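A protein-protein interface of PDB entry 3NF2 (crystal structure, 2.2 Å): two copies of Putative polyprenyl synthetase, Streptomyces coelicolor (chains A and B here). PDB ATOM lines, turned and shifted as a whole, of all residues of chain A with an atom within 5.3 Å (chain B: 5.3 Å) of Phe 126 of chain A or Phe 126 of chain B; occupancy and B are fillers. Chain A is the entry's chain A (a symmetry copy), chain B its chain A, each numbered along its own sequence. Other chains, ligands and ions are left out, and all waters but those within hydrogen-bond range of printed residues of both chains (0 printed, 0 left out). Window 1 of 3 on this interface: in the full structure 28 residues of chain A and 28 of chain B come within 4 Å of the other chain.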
ATOM      1  N   LEU A  85      13.902  -5.832  17.981  1.00  0.00           N
ATOM      2  CA  LEU A  85      14.041  -7.155  17.392  1.00  0.00           C
ATOM      3  C   LEU A  85      13.569  -8.245  18.348  1.00  0.00           C
ATOM      4  O   LEU A  85      12.798  -9.123  17.947  1.00  0.00           O
ATOM      5  CB  LEU A  85      15.486  -7.398  16.936  1.00  0.00           C
ATOM      6  CG  LEU A  85      15.892  -6.704  15.632  1.00  0.00           C
ATOM      7  CD1 LEU A  85      17.412  -6.755  15.428  1.00  0.00           C
ATOM      8  CD2 LEU A  85      15.163  -7.275  14.415  1.00  0.00           C
ATOM      9  N   VAL A  86      14.020  -8.163  19.605  1.00  0.00           N
ATOM     10  CA  VAL A  86      13.607  -9.092  20.665  1.00  0.00           C
ATOM     11  C   VAL A  86      12.109  -8.983  20.904  1.00  0.00           C
ATOM     12  O   VAL A  86      11.413 -10.009  21.024  1.00  0.00           O
ATOM     13  CB  VAL A  86      14.378  -8.851  21.990  1.00  0.00           C
ATOM     14  CG1 VAL A  86      13.737  -9.605  23.139  1.00  0.00           C
ATOM     15  CG2 VAL A  86      15.814  -9.306  21.858  1.00  0.00           C
ATOM     16  N   PHE A  89      10.409 -10.794  17.945  1.00  0.00           N
ATOM     17  CA  PHE A  89      10.622 -12.233  18.156  1.00  0.00           C
ATOM     18  C   PHE A  89       9.600 -12.753  19.146  1.00  0.00           C
ATOM     19  O   PHE A  89       8.995 -13.806  18.944  1.00  0.00           O
ATOM     20  CB  PHE A  89      12.072 -12.479  18.642  1.00  0.00           C
ATOM     21  CG  PHE A  89      12.206 -13.453  19.809  1.00  0.00           C
ATOM     22  CD1 PHE A  89      12.472 -12.981  21.094  1.00  0.00           C
ATOM     23  CD2 PHE A  89      12.125 -14.836  19.614  1.00  0.00           C
ATOM     24  CE1 PHE A  89      12.617 -13.863  22.181  1.00  0.00           C
ATOM     25  CE2 PHE A  89      12.276 -15.730  20.691  1.00  0.00           C
ATOM     26  CZ  PHE A  89      12.515 -15.240  21.977  1.00  0.00           C
ATOM     27  N   VAL A 121      11.578 -17.252  11.623  1.00  0.00           N
ATOM     28  CA  VAL A 121      11.828 -15.812  11.592  1.00  0.00           C
ATOM     29  C   VAL A 121      11.920 -15.226  13.014  1.00  0.00           C
ATOM     30  O   VAL A 121      12.783 -14.402  13.300  1.00  0.00           O
ATOM     31  CB  VAL A 121      10.797 -15.085  10.698  1.00  0.00           C
ATOM     32  CG1 VAL A 121      11.056 -13.596  10.689  1.00  0.00           C
ATOM     33  CG2 VAL A 121      10.891 -15.619   9.263  1.00  0.00           C
ATOM     34  N   GLY A 122      11.062 -15.693  13.908  1.00  0.00           N
ATOM     35  CA  GLY A 122      11.200 -15.381  15.328  1.00  0.00           C
ATOM     36  C   GLY A 122      12.601 -15.645  15.843  1.00  0.00           C
ATOM     37  O   GLY A 122      13.243 -14.730  16.399  1.00  0.00           O
ATOM     38  N   ASP A 123      13.093 -16.876  15.644  1.00  0.00           N
ATOM     39  CA  ASP A 123      14.468 -17.223  16.042  1.00  0.00           C
ATOM     40  C   ASP A 123      15.525 -16.325  15.398  1.00  0.00           C
ATOM     41  O   ASP A 123      16.521 -15.978  16.027  1.00  0.00           O
ATOM     42  CB  ASP A 123      14.795 -18.676  15.685  1.00  0.00           C
ATOM     43  CG  ASP A 123      14.047 -19.668  16.536  1.00  0.00           C
ATOM     44  OD1 ASP A 123      13.564 -19.288  17.618  1.00  0.00           O
ATOM     45  OD2 ASP A 123      13.943 -20.842  16.127  1.00  0.00           O
ATOM     46  N   ALA A 124      15.308 -15.990  14.128  1.00  0.00           N
ATOM     47  CA  ALA A 124      16.261 -15.226  13.361  1.00  0.00           C
ATOM     48  C   ALA A 124      16.371 -13.809  13.901  1.00  0.00           C
ATOM     49  O   ALA A 124      17.464 -13.271  13.968  1.00  0.00           O
ATOM     50  CB  ALA A 124      15.866 -15.209  11.902  1.00  0.00           C
ATOM     51  N   LEU A 125      15.239 -13.228  14.301  1.00  0.00           N
ATOM     52  CA  LEU A 125      15.215 -11.884  14.881  1.00  0.00           C
ATOM     53  C   LEU A 125      15.917 -11.833  16.234  1.00  0.00           C
ATOM     54  O   LEU A 125      16.629 -10.873  16.536  1.00  0.00           O
ATOM     55  CB  LEU A 125      13.779 -11.355  15.000  1.00  0.00           C
ATOM     56  CG  LEU A 125      12.952 -11.054  13.735  1.00  0.00           C
ATOM     57  CD1 LEU A 125      11.654 -10.341  14.114  1.00  0.00           C
ATOM     58  CD2 LEU A 125      13.698 -10.242  12.687  1.00  0.00           C
ATOM     59  N   PHE A 126      15.724 -12.880  17.037  1.00  0.00           N
ATOM     60  CA  PHE A 126      16.359 -12.980  18.343  1.00  0.00           C
ATOM     61  C   PHE A 126      17.879 -13.153  18.212  1.00  0.00           C
ATOM     62  O   PHE A 126      18.644 -12.547  18.970  1.00  0.00           O
ATOM     63  CB  PHE A 126      15.715 -14.102  19.178  1.00  0.00           C
ATOM     64  CG  PHE A 126      16.248 -14.211  20.595  1.00  0.00           C
ATOM     65  CD1 PHE A 126      16.672 -13.088  21.314  1.00  0.00           C
ATOM     66  CD2 PHE A 126      16.276 -15.438  21.230  1.00  0.00           C
ATOM     67  CE1 PHE A 126      17.165 -13.211  22.617  1.00  0.00           C
ATOM     68  CE2 PHE A 126      16.766 -15.569  22.535  1.00  0.00           C
ATOM     69  CZ  PHE A 126      17.212 -14.449  23.225  1.00  0.00           C
ATOM     70  N   ALA A 127      18.319 -13.949  17.245  1.00  0.00           N
ATOM     71  CA  ALA A 127      19.758 -14.066  16.990  1.00  0.00           C
ATOM     72  C   ALA A 127      20.353 -12.772  16.398  1.00  0.00           C
ATOM     73  O   ALA A 127      21.484 -12.392  16.732  1.00  0.00           O
ATOM     74  CB  ALA A 127      20.057 -15.256  16.104  1.00  0.00           C
ATOM     75  N   LEU A 128      19.584 -12.095  15.544  1.00  0.00           N
ATOM     76  CA  LEU A 128      20.022 -10.826  14.949  1.00  0.00           C
ATOM     77  C   LEU A 128      20.205  -9.702  15.978  1.00  0.00           C
ATOM     78  O   LEU A 128      21.049  -8.821  15.803  1.00  0.00           O
ATOM     79  CB  LEU A 128      19.046 -10.385  13.843  1.00  0.00           C
ATOM     80  CG  LEU A 128      19.416  -9.187  12.967  1.00  0.00           C
ATOM     81  CD1 LEU A 128      20.771  -9.350  12.226  1.00  0.00           C
ATOM     82  CD2 LEU A 128      18.309  -8.914  11.987  1.00  0.00           C
ATOM     83  N   ALA A 129      19.403  -9.744  17.040  1.00  0.00           N
ATOM     84  CA  ALA A 129      19.421  -8.718  18.079  1.00  0.00           C
ATOM     85  C   ALA A 129      20.726  -8.767  18.823  1.00  0.00           C
ATOM     86  O   ALA A 129      21.341  -7.728  19.077  1.00  0.00           O
ATOM     87  CB  ALA A 129      18.252  -8.909  19.048  1.00  0.00           C
ATOM     88  N   ASN A 130      21.144  -9.982  19.162  1.00  0.00           N
ATOM     89  CA  ASN A 130      22.429 -10.219  19.803  1.00  0.00           C
ATOM     90  C   ASN A 130      23.591  -9.828  18.899  1.00  0.00           C
ATOM     91  O   ASN A 130      24.601  -9.309  19.374  1.00  0.00           O
ATOM     92  CB  ASN A 130      22.561 -11.691  20.211  1.00  0.00           C
ATOM     93  CG  ASN A 130      21.614 -12.071  21.320  1.00  0.00           C
ATOM     94  OD1 ASN A 130      21.414 -11.319  22.262  1.00  0.00           O
ATOM     95  ND2 ASN A 130      21.032 -13.251  21.217  1.00  0.00           N
ATOM     96  N   SER A 152      15.158 -10.791  27.895  1.00  0.00           N
ATOM     97  CA  SER A 152      14.630 -11.793  26.986  1.00  0.00           C
ATOM     98  C   SER A 152      14.258 -13.047  27.755  1.00  0.00           C
ATOM     99  O   SER A 152      13.218 -13.637  27.483  1.00  0.00           O
ATOM    100  CB  SER A 152      15.633 -12.106  25.879  1.00  0.00           C
ATOM    101  OG  SER A 152      16.766 -12.749  26.427  1.00  0.00           O
ATOM    102  N   ILE A 156      10.340 -14.601  28.178  1.00  0.00           N
ATOM    103  CA  ILE A 156      10.088 -16.038  28.045  1.00  0.00           C
ATOM    104  C   ILE A 156       9.399 -16.553  29.317  1.00  0.00           C
ATOM    105  O   ILE A 156       8.392 -17.276  29.227  1.00  0.00           O
ATOM    106  CB  ILE A 156      11.395 -16.821  27.717  1.00  0.00           C
ATOM    107  CG1 ILE A 156      11.898 -16.461  26.314  1.00  0.00           C
ATOM    108  CG2 ILE A 156      11.175 -18.314  27.807  1.00  0.00           C
ATOM    109  CD1 ILE A 156      13.404 -16.625  26.149  1.00  0.00           C
ATOM    110  N   LEU B  85      23.276 -26.110  24.611  1.00  0.00           N
ATOM    111  CA  LEU B  85      21.991 -25.452  24.786  1.00  0.00           C
ATOM    112  C   LEU B  85      21.427 -24.962  23.456  1.00  0.00           C
ATOM    113  O   LEU B  85      20.254 -25.212  23.155  1.00  0.00           O
ATOM    114  CB  LEU B  85      22.098 -24.308  25.802  1.00  0.00           C
ATOM    115  CG  LEU B  85      22.154 -24.734  27.273  1.00  0.00           C
ATOM    116  CD1 LEU B  85      22.564 -23.563  28.174  1.00  0.00           C
ATOM    117  CD2 LEU B  85      20.837 -25.350  27.751  1.00  0.00           C
ATOM    118  N   VAL B  86      22.274 -24.292  22.667  1.00  0.00           N
ATOM    119  CA  VAL B  86      21.911 -23.813  21.328  1.00  0.00           C
ATOM    120  C   VAL B  86      21.571 -24.989  20.424  1.00  0.00           C
ATOM    121  O   VAL B  86      20.566 -24.950  19.690  1.00  0.00           O
ATOM    122  CB  VAL B  86      23.033 -22.954  20.686  1.00  0.00           C
ATOM    123  CG1 VAL B  86      22.770 -22.726  19.210  1.00  0.00           C
ATOM    124  CG2 VAL B  86      23.130 -21.610  21.371  1.00  0.00           C
ATOM    125  N   PHE B  89      18.064 -26.199  21.504  1.00  0.00           N
ATOM    126  CA  PHE B  89      17.107 -25.192  21.024  1.00  0.00           C
ATOM    127  C   PHE B  89      16.811 -25.437  19.559  1.00  0.00           C
ATOM    128  O   PHE B  89      15.659 -25.402  19.126  1.00  0.00           O
ATOM    129  CB  PHE B  89      17.678 -23.773  21.268  1.00  0.00           C
ATOM    130  CG  PHE B  89      17.531 -22.806  20.097  1.00  0.00           C
ATOM    131  CD1 PHE B  89      18.633 -22.484  19.305  1.00  0.00           C
ATOM    132  CD2 PHE B  89      16.311 -22.179  19.822  1.00  0.00           C
ATOM    133  CE1 PHE B  89      18.524 -21.582  18.231  1.00  0.00           C
ATOM    134  CE2 PHE B  89      16.189 -21.269  18.755  1.00  0.00           C
ATOM    135  CZ  PHE B  89      17.296 -20.976  17.955  1.00  0.00           C
ATOM    136  N   VAL B 121      10.268 -23.587  25.434  1.00  0.00           N
ATOM    137  CA  VAL B 121      11.484 -24.176  25.994  1.00  0.00           C
ATOM    138  C   VAL B 121      12.680 -24.015  25.037  1.00  0.00           C
ATOM    139  O   VAL B 121      13.786 -23.696  25.461  1.00  0.00           O
ATOM    140  CB  VAL B 121      11.244 -25.641  26.429  1.00  0.00           C
ATOM    141  CG1 VAL B 121      12.512 -26.244  26.989  1.00  0.00           C
ATOM    142  CG2 VAL B 121      10.150 -25.687  27.503  1.00  0.00           C
ATOM    143  N   GLY B 122      12.439 -24.186  23.746  1.00  0.00           N
ATOM    144  CA  GLY B 122      13.435 -23.839  22.736  1.00  0.00           C
ATOM    145  C   GLY B 122      13.988 -22.441  22.926  1.00  0.00           C
ATOM    146  O   GLY B 122      15.219 -22.269  23.046  1.00  0.00           O
ATOM    147  N   ASP B 123      13.095 -21.443  22.980  1.00  0.00           N
ATOM    148  CA  ASP B 123      13.516 -20.054  23.230  1.00  0.00           C
ATOM    149  C   ASP B 123      14.293 -19.888  24.537  1.00  0.00           C
ATOM    150  O   ASP B 123      15.239 -19.107  24.609  1.00  0.00           O
ATOM    151  CB  ASP B 123      12.309 -19.112  23.270  1.00  0.00           C
ATOM    152  CG  ASP B 123      11.672 -18.923  21.919  1.00  0.00           C
ATOM    153  OD1 ASP B 123      12.330 -19.202  20.900  1.00  0.00           O
ATOM    154  OD2 ASP B 123      10.504 -18.487  21.868  1.00  0.00           O
ATOM    155  N   ALA B 124      13.855 -20.603  25.570  1.00  0.00           N
ATOM    156  CA  ALA B 124      14.428 -20.482  26.888  1.00  0.00           C
ATOM    157  C   ALA B 124      15.854 -21.006  26.903  1.00  0.00           C
ATOM    158  O   ALA B 124      16.711 -20.414  27.539  1.00  0.00           O
ATOM    159  CB  ALA B 124      13.580 -21.220  27.898  1.00  0.00           C
ATOM    160  N   LEU B 125      16.099 -22.102  26.183  1.00  0.00           N
ATOM    161  CA  LEU B 125      17.440 -22.683  26.077  1.00  0.00           C
ATOM    162  C   LEU B 125      18.401 -21.768  25.324  1.00  0.00           C
ATOM    163  O   LEU B 125      19.567 -21.638  25.701  1.00  0.00           O
ATOM    164  CB  LEU B 125      17.395 -24.071  25.425  1.00  0.00           C
ATOM    165  CG  LEU B 125      16.711 -25.249  26.143  1.00  0.00           C
ATOM    166  CD1 LEU B 125      16.990 -26.553  25.396  1.00  0.00           C
ATOM    167  CD2 LEU B 125      17.108 -25.397  27.604  1.00  0.00           C
ATOM    168  N   PHE B 126      17.899 -21.125  24.271  1.00  0.00           N
ATOM    169  CA  PHE B 126      18.693 -20.196  23.480  1.00  0.00           C
ATOM    170  C   PHE B 126      19.043 -18.937  24.287  1.00  0.00           C
ATOM    171  O   PHE B 126      20.173 -18.443  24.214  1.00  0.00           O
ATOM    172  CB  PHE B 126      17.982 -19.860  22.157  1.00  0.00           C
ATOM    173  CG  PHE B 126      18.787 -18.975  21.222  1.00  0.00           C
ATOM    174  CD1 PHE B 126      20.182 -19.041  21.160  1.00  0.00           C
ATOM    175  CD2 PHE B 126      18.138 -18.108  20.364  1.00  0.00           C
ATOM    176  CE1 PHE B 126      20.906 -18.212  20.297  1.00  0.00           C
ATOM    177  CE2 PHE B 126      18.855 -17.276  19.494  1.00  0.00           C
ATOM    178  CZ  PHE B 126      20.242 -17.333  19.466  1.00  0.00           C
ATOM    179  N   ALA B 127      18.097 -18.434  25.071  1.00  0.00           N
ATOM    180  CA  ALA B 127      18.401 -17.306  25.956  1.00  0.00           C
ATOM    181  C   ALA B 127      19.350 -17.704  27.105  1.00  0.00           C
ATOM    182  O   ALA B 127      20.226 -16.920  27.495  1.00  0.00           O
ATOM    183  CB  ALA B 127      17.133 -16.678  26.492  1.00  0.00           C
ATOM    184  N   LEU B 128      19.186 -18.923  27.622  1.00  0.00           N
ATOM    185  CA  LEU B 128      20.057 -19.432  28.689  1.00  0.00           C
ATOM    186  C   LEU B 128      21.518 -19.601  28.254  1.00  0.00           C
ATOM    187  O   LEU B 128      22.436 -19.460  29.065  1.00  0.00           O
ATOM    188  CB  LEU B 128      19.506 -20.759  29.245  1.00  0.00           C
ATOM    189  CG  LEU B 128      20.158 -21.364  30.489  1.00  0.00           C
ATOM    190  CD1 LEU B 128      20.156 -20.415  31.719  1.00  0.00           C
ATOM    191  CD2 LEU B 128      19.490 -22.667  30.828  1.00  0.00           C
ATOM    192  N   ALA B 129      21.718 -19.910  26.974  1.00  0.00           N
ATOM    193  CA  ALA B 129      23.045 -20.154  26.421  1.00  0.00           C
ATOM    194  C   ALA B 129      23.848 -18.883  26.439  1.00  0.00           C
ATOM    195  O   ALA B 129      25.018 -18.886  26.828  1.00  0.00           O
ATOM    196  CB  ALA B 129      22.947 -20.699  24.995  1.00  0.00           C
ATOM    197  N   ASN B 130      23.204 -17.798  26.018  1.00  0.00           N
ATOM    198  CA  ASN B 130      23.800 -16.470  26.056  1.00  0.00           C
ATOM    199  C   ASN B 130      24.087 -16.020  27.482  1.00  0.00           C
ATOM    200  O   ASN B 130      25.096 -15.367  27.737  1.00  0.00           O
ATOM    201  CB  ASN B 130      22.884 -15.453  25.364  1.00  0.00           C
ATOM    202  CG  ASN B 130      22.785 -15.680  23.878  1.00  0.00           C
ATOM    203  OD1 ASN B 130      23.770 -15.976  23.220  1.00  0.00           O
ATOM    204  ND2 ASN B 130      21.589 -15.532  23.339  1.00  0.00           N
ATOM    205  N   SER B 152      24.688 -19.602  15.659  1.00  0.00           N
ATOM    206  CA  SER B 152      23.256 -19.737  15.861  1.00  0.00           C
ATOM    207  C   SER B 152      22.507 -19.134  14.687  1.00  0.00           C
ATOM    208  O   SER B 152      21.529 -19.716  14.231  1.00  0.00           O
ATOM    209  CB  SER B 152      22.828 -19.090  17.176  1.00  0.00           C
ATOM    210  OG  SER B 152      23.000 -17.690  17.099  1.00  0.00           O
ATOM    211  N   ILE B 156      20.064 -21.271  11.968  1.00  0.00           N
ATOM    212  CA  ILE B 156      18.769 -20.732  11.543  1.00  0.00           C
ATOM    213  C   ILE B 156      18.738 -20.635  10.010  1.00  0.00           C
ATOM    214  O   ILE B 156      17.756 -21.066   9.383  1.00  0.00           O
ATOM    215  CB  ILE B 156      18.463 -19.368  12.232  1.00  0.00           C
ATOM    216  CG1 ILE B 156      18.240 -19.565  13.736  1.00  0.00           C
ATOM    217  CG2 ILE B 156      17.247 -18.709  11.623  1.00  0.00           C
ATOM    218  CD1 ILE B 156      18.576 -18.333  14.566  1.00  0.00           C
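The backbone carbonyl oxygen (O) of Phe 126 of chain B sits at hydrogen-bond distance from the side-chain amide nitrogen (ND2) of Asn 130 of chain B, at 3.4 Å. The backbone carbonyl oxygen (O) of Phe 126 of chain A is in hydrogen-bond range of the side-chain amide nitrogen (ND2) of Asn 130 of chain A (3.4 Å).
Phe 89 of chain A touches Asp 123 of chain B (CE2 to CG, 3.5 Å). Asp 123 of chain A touches Phe 89 of chain B. Asp 123 of chain A touches Asp 123 of chain B. Phe 126 of chain B touches Phe 126 of chain A. CZ of Phe 126 of chain A touches CB of Ala 127 of chain B, 3.96 Å away. Ala 127 of chain A touches Phe 126 of chain B. OG of Ser 152 of chain A touches CB of Ala 127 of chain B (3.9 Å). O of Asp 123 of chain B touches CD1 of Ile 156 of chain A, at 3.4 Å. CB of Ala 124 of chain B touches CG2 of Ile 156 of chain A, at 3.8 Å. CD1 of Ile 156 of chain A touches CB of Ala 127 of chain B, 3.7 Å away.
The side-chain amide nitrogen of Asn 130 of chain B sits close to the side-chain amide nitrogen of Asn 130 of chain A (3.2 Å).
Phe 89 of chain A touches Asp 123 of chain B, and with the chains exchanged Asp 123 of chain A touches Phe 89 of chain B. Asp 123 of chain A touches Ile 156 of chain B, and with the chains exchanged Ile 156 of chain A touches Asp 123 of chain B. Ala 124 of chain A touches Ile 156 of chain B, and with the chains exchanged Ile 156 of chain A touches Ala 124 of chain B. Asn 130 of chain A touches its own counterpart, Asn 130 of chain B. Positions printed for both chains: 85, 86, 89, 121, 122, 123, 124, 125, 126, 127, 128, 129, 130, 152 and 156. Of the 15 pairs that touch across the chains among the printed residues, 15 have their exchanged pair printed and touching as well.
Phe 126 of chain A touches just these residues of chain B: Phe 126 (3.4 Å) and Ala 127 (3.96 Å). Printed residues of chain B within 4 Å of Ser 152 of chain A: Ala 127 (3.9 Å). Leu 85 of chain B touches none of the printed residues of chain A. Leu 125 of chain B touches none of the printed residues of chain A. Phe 126 of chain B touches two residues of chain A. Printed residues of chain A within 4 Å of Ala 127 of chain B: Phe 126 (3.96 Å), Ser 152 (3.9 Å) and Ile 156 (3.7 Å). The nearest residue of chain B that does not touch Phe 126 of chain A is Asp 123 of chain B (4.4 Å). The nearest residue of chain A that does not touch Phe 126 of chain B is Asp 123 of chain A (4.4 Å).
Of the 15 printed residues of chain B, 8 touch a printed residue of chain A. Among the printed residues, 15 pairs touch across the chains. Among the printed residues, no Asp or Glu carboxylate lies within 4 Å of a Lys or Arg side-chain nitrogen of the other chain.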
